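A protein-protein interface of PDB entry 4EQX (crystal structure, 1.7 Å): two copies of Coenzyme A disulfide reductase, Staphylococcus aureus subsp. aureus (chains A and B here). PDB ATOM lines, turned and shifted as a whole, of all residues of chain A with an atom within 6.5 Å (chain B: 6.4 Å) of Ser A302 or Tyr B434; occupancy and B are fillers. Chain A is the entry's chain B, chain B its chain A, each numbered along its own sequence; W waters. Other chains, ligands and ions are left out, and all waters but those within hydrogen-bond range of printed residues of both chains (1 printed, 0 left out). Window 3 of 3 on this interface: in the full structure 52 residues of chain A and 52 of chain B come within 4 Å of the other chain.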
ATOM      1  N   THR A  14      -1.293 -13.426  36.582  1.00  0.00           N
ATOM      2  CA  THR A  14      -0.423 -14.374  35.851  1.00  0.00           C
ATOM      3  C   THR A  14      -0.168 -13.963  34.422  1.00  0.00           C
ATOM      4  O   THR A  14       0.951 -14.034  33.950  1.00  0.00           O
ATOM      5  CB  THR A  14      -1.081 -15.757  35.861  1.00  0.00           C
ATOM      6  OG1 THR A  14      -1.364 -16.068  37.260  1.00  0.00           O
ATOM      7  CG2 THR A  14      -0.168 -16.847  35.231  1.00  0.00           C
ATOM      8  N   CYS A  15      -1.224 -13.573  33.733  1.00  0.00           N
ATOM      9  CA  CYS A  15      -1.070 -13.227  32.308  1.00  0.00           C
ATOM     10  C   CYS A  15      -0.157 -11.987  32.205  1.00  0.00           C
ATOM     11  O   CYS A  15       0.761 -11.997  31.371  1.00  0.00           O
ATOM     12  CB  CYS A  15      -2.497 -13.010  31.624  1.00  0.00           C
ATOM     13  SG  CYS A  15      -2.298 -12.701  29.882  1.00  0.00           S
ATOM     14  N   GLN A  18       3.416 -12.907  32.756  1.00  0.00           N
ATOM     15  CA  GLN A  18       3.959 -13.655  31.645  1.00  0.00           C
ATOM     16  C   GLN A  18       4.251 -12.734  30.481  1.00  0.00           C
ATOM     17  O   GLN A  18       5.220 -12.953  29.718  1.00  0.00           O
ATOM     18  CB  GLN A  18       2.970 -14.756  31.223  1.00  0.00           C
ATOM     19  CG  GLN A  18       2.906 -15.872  32.325  1.00  0.00           C
ATOM     20  CD  GLN A  18       4.095 -16.780  32.252  1.00  0.00           C
ATOM     21  OE1 GLN A  18       4.291 -17.485  31.281  1.00  0.00           O
ATOM     22  NE2 GLN A  18       4.937 -16.688  33.229  1.00  0.00           N
ATOM     23  N   LEU A  22       8.256 -11.606  28.548  1.00  0.00           N
ATOM     24  CA  LEU A  22       8.567 -11.494  27.133  1.00  0.00           C
ATOM     25  C   LEU A  22       8.775 -10.060  26.631  1.00  0.00           C
ATOM     26  O   LEU A  22       9.490  -9.844  25.625  1.00  0.00           O
ATOM     27  CB  LEU A  22       7.429 -12.058  26.302  1.00  0.00           C
ATOM     28  CG  LEU A  22       7.271 -13.561  26.521  1.00  0.00           C
ATOM     29  CD1 LEU A  22       5.829 -13.823  26.085  1.00  0.00           C
ATOM     30  CD2 LEU A  22       8.253 -14.350  25.654  1.00  0.00           C
ATOM     31  N   TRP A 295      -5.794 -24.632  36.657  1.00  0.00           N
ATOM     32  CA  TRP A 295      -4.886 -24.997  35.519  1.00  0.00           C
ATOM     33  C   TRP A 295      -5.207 -24.231  34.249  1.00  0.00           C
ATOM     34  O   TRP A 295      -4.284 -23.755  33.574  1.00  0.00           O
ATOM     35  CB  TRP A 295      -4.980 -26.530  35.263  1.00  0.00           C
ATOM     36  CG  TRP A 295      -4.032 -26.932  34.201  1.00  0.00           C
ATOM     37  CD1 TRP A 295      -2.733 -27.289  34.357  1.00  0.00           C
ATOM     38  CD2 TRP A 295      -4.321 -26.966  32.808  1.00  0.00           C
ATOM     39  NE1 TRP A 295      -2.175 -27.548  33.115  1.00  0.00           N
ATOM     40  CE2 TRP A 295      -3.132 -27.386  32.153  1.00  0.00           C
ATOM     41  CE3 TRP A 295      -5.483 -26.746  32.060  1.00  0.00           C
ATOM     42  CZ2 TRP A 295      -3.068 -27.521  30.719  1.00  0.00           C
ATOM     43  CZ3 TRP A 295      -5.471 -26.932  30.697  1.00  0.00           C
ATOM     44  CH2 TRP A 295      -4.251 -27.302  30.021  1.00  0.00           C
ATOM     45  N   ALA A 297      -6.815 -21.341  33.918  1.00  0.00           N
ATOM     46  CA  ALA A 297      -6.577 -19.889  34.010  1.00  0.00           C
ATOM     47  C   ALA A 297      -5.057 -19.666  33.740  1.00  0.00           C
ATOM     48  O   ALA A 297      -4.650 -18.697  32.996  1.00  0.00           O
ATOM     49  CB  ALA A 297      -6.975 -19.372  35.440  1.00  0.00           C
ATOM     50  N   HIS A 298      -4.208 -20.491  34.356  1.00  0.00           N
ATOM     51  CA  HIS A 298      -2.771 -20.388  34.155  1.00  0.00           C
ATOM     52  C   HIS A 298      -2.289 -20.769  32.744  1.00  0.00           C
ATOM     53  O   HIS A 298      -1.421 -20.064  32.174  1.00  0.00           O
ATOM     54  CB  HIS A 298      -2.016 -21.212  35.213  1.00  0.00           C
ATOM     55  CG  HIS A 298      -2.071 -20.582  36.527  1.00  0.00           C
ATOM     56  ND1 HIS A 298      -0.956 -20.051  37.137  1.00  0.00           N
ATOM     57  CD2 HIS A 298      -3.114 -20.366  37.360  1.00  0.00           C
ATOM     58  CE1 HIS A 298      -1.323 -19.579  38.313  1.00  0.00           C
ATOM     59  NE2 HIS A 298      -2.617 -19.702  38.444  1.00  0.00           N
ATOM     60  N   ARG A 299      -2.917 -21.763  32.138  1.00  0.00           N
ATOM     61  CA  ARG A 299      -2.438 -22.142  30.826  1.00  0.00           C
ATOM     62  C   ARG A 299      -2.893 -21.084  29.834  1.00  0.00           C
ATOM     63  O   ARG A 299      -2.095 -20.685  28.955  1.00  0.00           O
ATOM     64  CB  ARG A 299      -3.049 -23.525  30.441  1.00  0.00           C
ATOM     65  CG  ARG A 299      -2.841 -23.926  28.902  1.00  0.00           C
ATOM     66  CD  ARG A 299      -1.274 -24.204  28.814  1.00  0.00           C
ATOM     67  NE  ARG A 299      -0.965 -24.473  27.425  1.00  0.00           N
ATOM     68  CZ  ARG A 299       0.137 -24.068  26.792  1.00  0.00           C
ATOM     69  NH1 ARG A 299       0.274 -24.334  25.458  1.00  0.00           N
ATOM     70  NH2 ARG A 299       1.104 -23.470  27.457  1.00  0.00           N
ATOM     71  N   ALA A 300      -4.160 -20.627  29.936  1.00  0.00           N
ATOM     72  CA  ALA A 300      -4.615 -19.491  29.046  1.00  0.00           C
ATOM     73  C   ALA A 300      -3.751 -18.228  29.230  1.00  0.00           C
ATOM     74  O   ALA A 300      -3.486 -17.495  28.276  1.00  0.00           O
ATOM     75  CB  ALA A 300      -6.084 -19.142  29.353  1.00  0.00           C
ATOM     76  N   ALA A 301      -3.418 -17.928  30.508  1.00  0.00           N
ATOM     77  CA  ALA A 301      -2.562 -16.732  30.750  1.00  0.00           C
ATOM     78  C   ALA A 301      -1.279 -16.860  29.908  1.00  0.00           C
ATOM     79  O   ALA A 301      -0.830 -15.902  29.254  1.00  0.00           O
ATOM     80  CB  ALA A 301      -2.279 -16.610  32.276  1.00  0.00           C
ATOM     81  N   SER A 302      -0.619 -18.037  29.952  1.00  0.00           N
ATOM     82  CA  SER A 302       0.579 -18.249  29.123  1.00  0.00           C
ATOM     83  C   SER A 302       0.380 -18.121  27.625  1.00  0.00           C
ATOM     84  O   SER A 302       1.198 -17.510  26.931  1.00  0.00           O
ATOM     85  CB  SER A 302       1.265 -19.592  29.432  1.00  0.00           C
ATOM     86  OG  SER A 302       1.509 -19.601  30.840  1.00  0.00           O
ATOM     87  N   ILE A 303      -0.662 -18.761  27.098  1.00  0.00           N
ATOM     88  CA  ILE A 303      -0.985 -18.698  25.651  1.00  0.00           C
ATOM     89  C   ILE A 303      -1.289 -17.281  25.219  1.00  0.00           C
ATOM     90  O   ILE A 303      -0.734 -16.865  24.193  1.00  0.00           O
ATOM     91  CB  ILE A 303      -2.188 -19.604  25.356  1.00  0.00           C
ATOM     92  CG1 ILE A 303      -1.702 -21.083  25.509  1.00  0.00           C
ATOM     93  CG2 ILE A 303      -2.764 -19.403  23.897  1.00  0.00           C
ATOM     94  CD1 ILE A 303      -2.897 -22.074  25.385  1.00  0.00           C
ATOM     95  N   VAL A 304      -2.112 -16.539  25.946  1.00  0.00           N
ATOM     96  CA  VAL A 304      -2.296 -15.122  25.654  1.00  0.00           C
ATOM     97  C   VAL A 304      -0.968 -14.321  25.675  1.00  0.00           C
ATOM     98  O   VAL A 304      -0.698 -13.482  24.742  1.00  0.00           O
ATOM     99  CB  VAL A 304      -3.386 -14.440  26.557  1.00  0.00           C
ATOM    100  CG1 VAL A 304      -3.438 -12.935  26.298  1.00  0.00           C
ATOM    101  CG2 VAL A 304      -4.727 -15.115  26.214  1.00  0.00           C
ATOM    102  N   ALA A 305      -0.130 -14.541  26.716  1.00  0.00           N
ATOM    103  CA  ALA A 305       1.174 -13.834  26.747  1.00  0.00           C
ATOM    104  C   ALA A 305       1.998 -14.158  25.446  1.00  0.00           C
ATOM    105  O   ALA A 305       2.560 -13.246  24.804  1.00  0.00           O
ATOM    106  CB  ALA A 305       1.963 -14.178  27.985  1.00  0.00           C
ATOM    107  N   GLU A 306       2.017 -15.418  25.037  1.00  0.00           N
ATOM    108  CA  GLU A 306       2.661 -15.771  23.722  1.00  0.00           C
ATOM    109  C   GLU A 306       2.013 -15.048  22.554  1.00  0.00           C
ATOM    110  O   GLU A 306       2.698 -14.528  21.673  1.00  0.00           O
ATOM    111  CB  GLU A 306       2.770 -17.274  23.498  1.00  0.00           C
ATOM    112  CG  GLU A 306       3.608 -17.937  24.594  1.00  0.00           C
ATOM    113  CD  GLU A 306       5.113 -17.808  24.511  1.00  0.00           C
ATOM    114  OE1 GLU A 306       5.669 -17.383  23.487  1.00  0.00           O
ATOM    115  OE2 GLU A 306       5.713 -18.095  25.579  1.00  0.00           O
ATOM    116  N   GLN A 307       0.681 -15.077  22.475  1.00  0.00           N
ATOM    117  CA  GLN A 307       0.003 -14.357  21.403  1.00  0.00           C
ATOM    118  C   GLN A 307       0.423 -12.911  21.289  1.00  0.00           C
ATOM    119  O   GLN A 307       0.685 -12.441  20.205  1.00  0.00           O
ATOM    120  CB  GLN A 307      -1.524 -14.463  21.584  1.00  0.00           C
ATOM    121  CG  GLN A 307      -2.089 -15.876  21.320  1.00  0.00           C
ATOM    122  CD  GLN A 307      -1.859 -16.371  19.857  1.00  0.00           C
ATOM    123  OE1 GLN A 307      -1.302 -17.489  19.599  1.00  0.00           O
ATOM    124  NE2 GLN A 307      -2.083 -15.524  18.960  1.00  0.00           N
ATOM    125  N   ILE A 314       1.624 -20.515  19.095  1.00  0.00           N
ATOM    126  CA  ILE A 314       1.193 -21.372  20.268  1.00  0.00           C
ATOM    127  C   ILE A 314      -0.307 -21.175  20.475  1.00  0.00           C
ATOM    128  O   ILE A 314      -0.766 -20.010  20.677  1.00  0.00           O
ATOM    129  CB  ILE A 314       2.032 -21.070  21.593  1.00  0.00           C
ATOM    130  CG1 ILE A 314       3.541 -21.359  21.302  1.00  0.00           C
ATOM    131  CG2 ILE A 314       1.357 -21.725  22.901  1.00  0.00           C
ATOM    132  CD1 ILE A 314       4.447 -20.860  22.413  1.00  0.00           C
ATOM    133  N   VAL B 408       9.140 -33.009  24.491  1.00  0.00           N
ATOM    134  CA  VAL B 408       9.309 -32.254  25.749  1.00  0.00           C
ATOM    135  C   VAL B 408       8.467 -30.980  25.692  1.00  0.00           C
ATOM    136  O   VAL B 408       7.926 -30.556  26.738  1.00  0.00           O
ATOM    137  CB  VAL B 408      10.815 -31.885  25.958  1.00  0.00           C
ATOM    138  CG1 VAL B 408      11.432 -30.984  24.840  1.00  0.00           C
ATOM    139  CG2 VAL B 408      11.050 -31.188  27.338  1.00  0.00           C
ATOM    140  N   ASP B 409       8.286 -30.430  24.468  1.00  0.00           N
ATOM    141  CA  ASP B 409       7.602 -29.136  24.425  1.00  0.00           C
ATOM    142  C   ASP B 409       6.130 -29.313  24.772  1.00  0.00           C
ATOM    143  O   ASP B 409       5.490 -28.398  25.327  1.00  0.00           O
ATOM    144  CB  ASP B 409       7.722 -28.506  23.023  1.00  0.00           C
ATOM    145  CG  ASP B 409       9.155 -28.346  22.617  1.00  0.00           C
ATOM    146  OD1 ASP B 409       9.818 -27.363  23.102  1.00  0.00           O
ATOM    147  OD2 ASP B 409       9.640 -29.233  21.887  1.00  0.00           O
ATOM    148  N   LEU B 411       4.852 -31.051  26.982  1.00  0.00           N
ATOM    149  CA  LEU B 411       4.535 -31.138  28.385  1.00  0.00           C
ATOM    150  C   LEU B 411       3.841 -29.864  28.917  1.00  0.00           C
ATOM    151  O   LEU B 411       3.188 -29.938  30.035  1.00  0.00           O
ATOM    152  CB  LEU B 411       5.805 -31.443  29.220  1.00  0.00           C
ATOM    153  CG  LEU B 411       6.511 -32.743  28.801  1.00  0.00           C
ATOM    154  CD1 LEU B 411       7.746 -32.869  29.727  1.00  0.00           C
ATOM    155  CD2 LEU B 411       5.526 -33.865  29.220  1.00  0.00           C
ATOM    156  N   THR B 412       4.044 -28.705  28.251  1.00  0.00           N
ATOM    157  CA  THR B 412       3.267 -27.533  28.685  1.00  0.00           C
ATOM    158  C   THR B 412       1.755 -27.768  28.653  1.00  0.00           C
ATOM    159  O   THR B 412       0.990 -27.083  29.343  1.00  0.00           O
ATOM    160  CB  THR B 412       3.578 -26.268  27.805  1.00  0.00           C
ATOM    161  OG1 THR B 412       3.214 -26.577  26.452  1.00  0.00           O
ATOM    162  CG2 THR B 412       5.044 -25.933  27.783  1.00  0.00           C
ATOM    163  N   GLU B 413       1.326 -28.716  27.830  1.00  0.00           N
ATOM    164  CA  GLU B 413      -0.083 -28.940  27.598  1.00  0.00           C
ATOM    165  C   GLU B 413      -0.729 -29.977  28.531  1.00  0.00           C
ATOM    166  O   GLU B 413      -1.995 -30.261  28.424  1.00  0.00           O
ATOM    167  CB  GLU B 413      -0.286 -29.509  26.179  1.00  0.00           C
ATOM    168  CG  GLU B 413       0.247 -28.507  25.091  1.00  0.00           C
ATOM    169  CD  GLU B 413       0.246 -29.117  23.745  1.00  0.00           C
ATOM    170  OE1 GLU B 413      -0.309 -30.221  23.594  1.00  0.00           O
ATOM    171  OE2 GLU B 413       0.884 -28.468  22.863  1.00  0.00           O
ATOM    172  N   LYS B 426       0.570 -24.815  37.582  1.00  0.00           N
ATOM    173  CA  LYS B 426       1.588 -25.242  36.598  1.00  0.00           C
ATOM    174  C   LYS B 426       2.366 -26.333  37.277  1.00  0.00           C
ATOM    175  O   LYS B 426       3.152 -26.060  38.189  1.00  0.00           O
ATOM    176  CB  LYS B 426       2.528 -24.072  36.178  1.00  0.00           C
ATOM    177  CG  LYS B 426       1.834 -22.902  35.537  1.00  0.00           C
ATOM    178  CD  LYS B 426       2.802 -21.795  35.059  1.00  0.00           C
ATOM    179  CE  LYS B 426       3.062 -20.630  36.076  1.00  0.00           C
ATOM    180  NZ  LYS B 426       1.877 -19.810  36.636  1.00  0.00           N
ATOM    181  N   ASP B 427       2.052 -27.583  36.959  1.00  0.00           N
ATOM    182  CA  ASP B 427       2.725 -28.716  37.705  1.00  0.00           C
ATOM    183  C   ASP B 427       4.204 -28.798  37.318  1.00  0.00           C
ATOM    184  O   ASP B 427       4.644 -28.248  36.296  1.00  0.00           O
ATOM    185  CB  ASP B 427       2.061 -30.057  37.298  1.00  0.00           C
ATOM    186  CG  ASP B 427       2.660 -31.208  38.078  1.00  0.00           C
ATOM    187  OD1 ASP B 427       3.173 -32.199  37.469  1.00  0.00           O
ATOM    188  OD2 ASP B 427       2.692 -31.004  39.360  1.00  0.00           O
ATOM    189  N   ILE B 429       5.651 -31.137  35.821  1.00  0.00           N
ATOM    190  CA  ILE B 429       5.687 -31.578  34.436  1.00  0.00           C
ATOM    191  C   ILE B 429       5.517 -30.395  33.448  1.00  0.00           C
ATOM    192  O   ILE B 429       6.268 -30.275  32.456  1.00  0.00           O
ATOM    193  CB  ILE B 429       4.644 -32.687  34.253  1.00  0.00           C
ATOM    194  CG1 ILE B 429       5.145 -33.961  34.961  1.00  0.00           C
ATOM    195  CG2 ILE B 429       4.446 -32.972  32.808  1.00  0.00           C
ATOM    196  CD1 ILE B 429       4.146 -35.100  34.985  1.00  0.00           C
ATOM    197  N   ASN B 430       4.518 -29.535  33.713  1.00  0.00           N
ATOM    198  CA  ASN B 430       4.361 -28.348  32.838  1.00  0.00           C
ATOM    199  C   ASN B 430       5.624 -27.476  32.834  1.00  0.00           C
ATOM    200  O   ASN B 430       6.030 -27.054  31.806  1.00  0.00           O
ATOM    201  CB  ASN B 430       3.182 -27.517  33.333  1.00  0.00           C
ATOM    202  CG  ASN B 430       1.854 -28.280  33.289  1.00  0.00           C
ATOM    203  OD1 ASN B 430       1.039 -28.187  34.265  1.00  0.00           O
ATOM    204  ND2 ASN B 430       1.544 -28.914  32.124  1.00  0.00           N
ATOM    205  N   MET B 431       6.210 -27.237  34.012  1.00  0.00           N
ATOM    206  CA  MET B 431       7.432 -26.400  34.128  1.00  0.00           C
ATOM    207  C   MET B 431       8.610 -26.904  33.291  1.00  0.00           C
ATOM    208  O   MET B 431       9.363 -26.102  32.696  1.00  0.00           O
ATOM    209  CB  MET B 431       7.843 -26.236  35.617  1.00  0.00           C
ATOM    210  CG  MET B 431       6.823 -25.389  36.449  1.00  0.00           C
ATOM    211  SD  MET B 431       6.396 -23.882  35.551  1.00  0.00           S
ATOM    212  CE  MET B 431       8.048 -23.314  34.974  1.00  0.00           C
ATOM    213  N   ILE B 432       8.805 -28.224  33.233  1.00  0.00           N
ATOM    214  CA  ILE B 432       9.754 -28.848  32.250  1.00  0.00           C
ATOM    215  C   ILE B 432       9.509 -28.312  30.807  1.00  0.00           C
ATOM    216  O   ILE B 432      10.441 -27.866  30.171  1.00  0.00           O
ATOM    217  CB  ILE B 432       9.765 -30.422  32.246  1.00  0.00           C
ATOM    218  CG1 ILE B 432      10.110 -31.008  33.661  1.00  0.00           C
ATOM    219  CG2 ILE B 432      10.646 -31.005  31.055  1.00  0.00           C
ATOM    220  CD1 ILE B 432      11.623 -30.745  34.020  1.00  0.00           C
ATOM    221  N   GLY B 433       8.249 -28.349  30.385  1.00  0.00           N
ATOM    222  CA  GLY B 433       7.855 -27.924  29.023  1.00  0.00           C
ATOM    223  C   GLY B 433       8.202 -26.431  28.892  1.00  0.00           C
ATOM    224  O   GLY B 433       8.837 -26.034  27.897  1.00  0.00           O
ATOM    225  N   TYR B 434       7.895 -25.628  29.929  1.00  0.00           N
ATOM    226  CA  TYR B 434       8.089 -24.162  29.796  1.00  0.00           C
ATOM    227  C   TYR B 434       9.580 -23.866  29.772  1.00  0.00           C
ATOM    228  O   TYR B 434       9.976 -22.874  29.180  1.00  0.00           O
ATOM    229  CB  TYR B 434       7.377 -23.350  30.871  1.00  0.00           C
ATOM    230  CG  TYR B 434       5.878 -23.366  30.747  1.00  0.00           C
ATOM    231  CD1 TYR B 434       5.090 -23.963  31.716  1.00  0.00           C
ATOM    232  CD2 TYR B 434       5.220 -22.744  29.633  1.00  0.00           C
ATOM    233  CE1 TYR B 434       3.709 -23.975  31.590  1.00  0.00           C
ATOM    234  CE2 TYR B 434       3.853 -22.795  29.521  1.00  0.00           C
ATOM    235  CZ  TYR B 434       3.097 -23.348  30.478  1.00  0.00           C
ATOM    236  OH  TYR B 434       1.714 -23.365  30.344  1.00  0.00           O
ATOM    237  N   LYS B 435      10.348 -24.715  30.433  1.00  0.00           N
ATOM    238  CA  LYS B 435      11.800 -24.506  30.617  1.00  0.00           C
ATOM    239  C   LYS B 435      12.651 -25.068  29.466  1.00  0.00           C
ATOM    240  O   LYS B 435      13.871 -24.827  29.419  1.00  0.00           O
ATOM    241  CB  LYS B 435      12.308 -25.080  31.966  1.00  0.00           C
ATOM    242  CG  LYS B 435      11.927 -24.321  33.192  1.00  0.00           C
ATOM    243  CD  LYS B 435      12.868 -24.766  34.421  1.00  0.00           C
ATOM    244  CE  LYS B 435      14.369 -24.567  34.083  1.00  0.00           C
ATOM    245  NZ  LYS B 435      15.324 -24.924  35.233  1.00  0.00           N
ATOM    246  N   ALA B 436      12.024 -25.653  28.438  1.00  0.00           N
ATOM    247  CA  ALA B 436      12.763 -26.398  27.443  1.00  0.00           C
ATOM    248  C   ALA B 436      13.067 -25.530  26.219  1.00  0.00           C
ATOM    249  O   ALA B 436      13.627 -26.007  25.226  1.00  0.00           O
ATOM    250  CB  ALA B 436      11.929 -27.643  26.981  1.00  0.00           C
ATOM    251  N   LYS B 437      12.604 -24.287  26.292  1.00  0.00           N
ATOM    252  CA  LYS B 437      12.859 -23.386  25.137  1.00  0.00           C
ATOM    253  C   LYS B 437      14.183 -22.587  25.146  1.00  0.00           C
ATOM    254  O   LYS B 437      15.156 -22.940  25.843  1.00  0.00           O
ATOM    255  CB  LYS B 437      11.601 -22.602  24.817  1.00  0.00           C
ATOM    256  CG  LYS B 437      10.494 -23.546  24.431  1.00  0.00           C
ATOM    257  CD  LYS B 437       9.271 -22.836  23.842  1.00  0.00           C
ATOM    258  CE  LYS B 437       8.570 -23.766  22.836  1.00  0.00           C
ATOM    259  NZ  LYS B 437       9.492 -24.888  22.328  1.00  0.00           N
ATOM    260  OXT LYS B 437      14.391 -21.622  24.378  1.00  0.00           O
HETATM  261  O   HOH W   1       3.317 -24.273  24.792  1.00  0.00           O
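NZ of Lys B426 lies within hydrogen-bond range of ND1 of His A298 (2.9 Å).
OD1 of Asn B430 lies within hydrogen-bond range of NE1 of Trp A295 (3.5 Å).
The side-chain hydroxyl (OH) of Tyr B434 lies within hydrogen-bond range of the guanidinium group (NH2) of Arg A299 (3.0 Å).
The side-chain hydroxyl (OG1) of Thr B412 lies within hydrogen-bond range of the backbone carbonyl oxygen (O) of Asp B409.
The side-chain amide nitrogen (ND2) of Asn B430 sits at hydrogen-bond distance from the backbone carbonyl oxygen (O) of Leu B411.
The backbone carbonyl oxygen (O) of Thr B412 is in hydrogen-bond range of the side-chain amide nitrogen (ND2) of Asn B430 (3.4 Å).
The backbone NH of Asp B427 sits at hydrogen-bond distance from the side-chain amide oxygen of Asn B430 (2.9 Å).
O of His A298 sits at hydrogen-bond distance from OG of Ser A302, 3.3 Å away.
CG2 of Thr A14 touches NZ of Lys B426, 3.9 Å away.
Glu B413 touches Trp A295 (O to CZ2, 3.7 Å).
Arg A299 touches Thr B412 (CD to O, 3.7 Å).
OH of Tyr B434 touches OG of Ser A302, at 3.8 Å.
Of the printed residues of chain B, Ser A302 touches Tyr B434.
Tyr B434 touches two residues of chain A.
Printed residues of chain B within 4 Å of Thr A14: Lys B426 (3.9 Å).
Printed residues of chain B within 4 Å of Trp A295: Glu B413 (3.7 Å) and Asn B430 (3.5 Å).
Gly B433 touches none of the printed residues of chain A.
The nearest printed residue of chain B that does not touch Ser A302 is Lys B426 (4.9 Å).
The nearest residue of chain A that does not touch Tyr B434 is His A298 (4.9 Å).
The nearest printed residue of chain B that does not touch Trp A295 is Thr B412 (4.3 Å).
Printed residues of chain B that touch a printed residue of chain A: Thr B412, Glu B413, Lys B426, Asn B430 and Tyr B434.
Hydrophobic or aromatic side chains of chain B that line the printed part of chain A: Tyr B434.
Among the printed residues, 7 pairs touch across the chains.
Among the printed residues, no Asp or Glu carboxylate lies within 4 Å of a Lys or Arg side-chain nitrogen of the other chain.
No position is printed for both chains.
Water W1 lies within hydrogen-bond range of OG1 of Thr B412 (2.8 Å) and NH1 of Arg A299 (3.1 Å).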
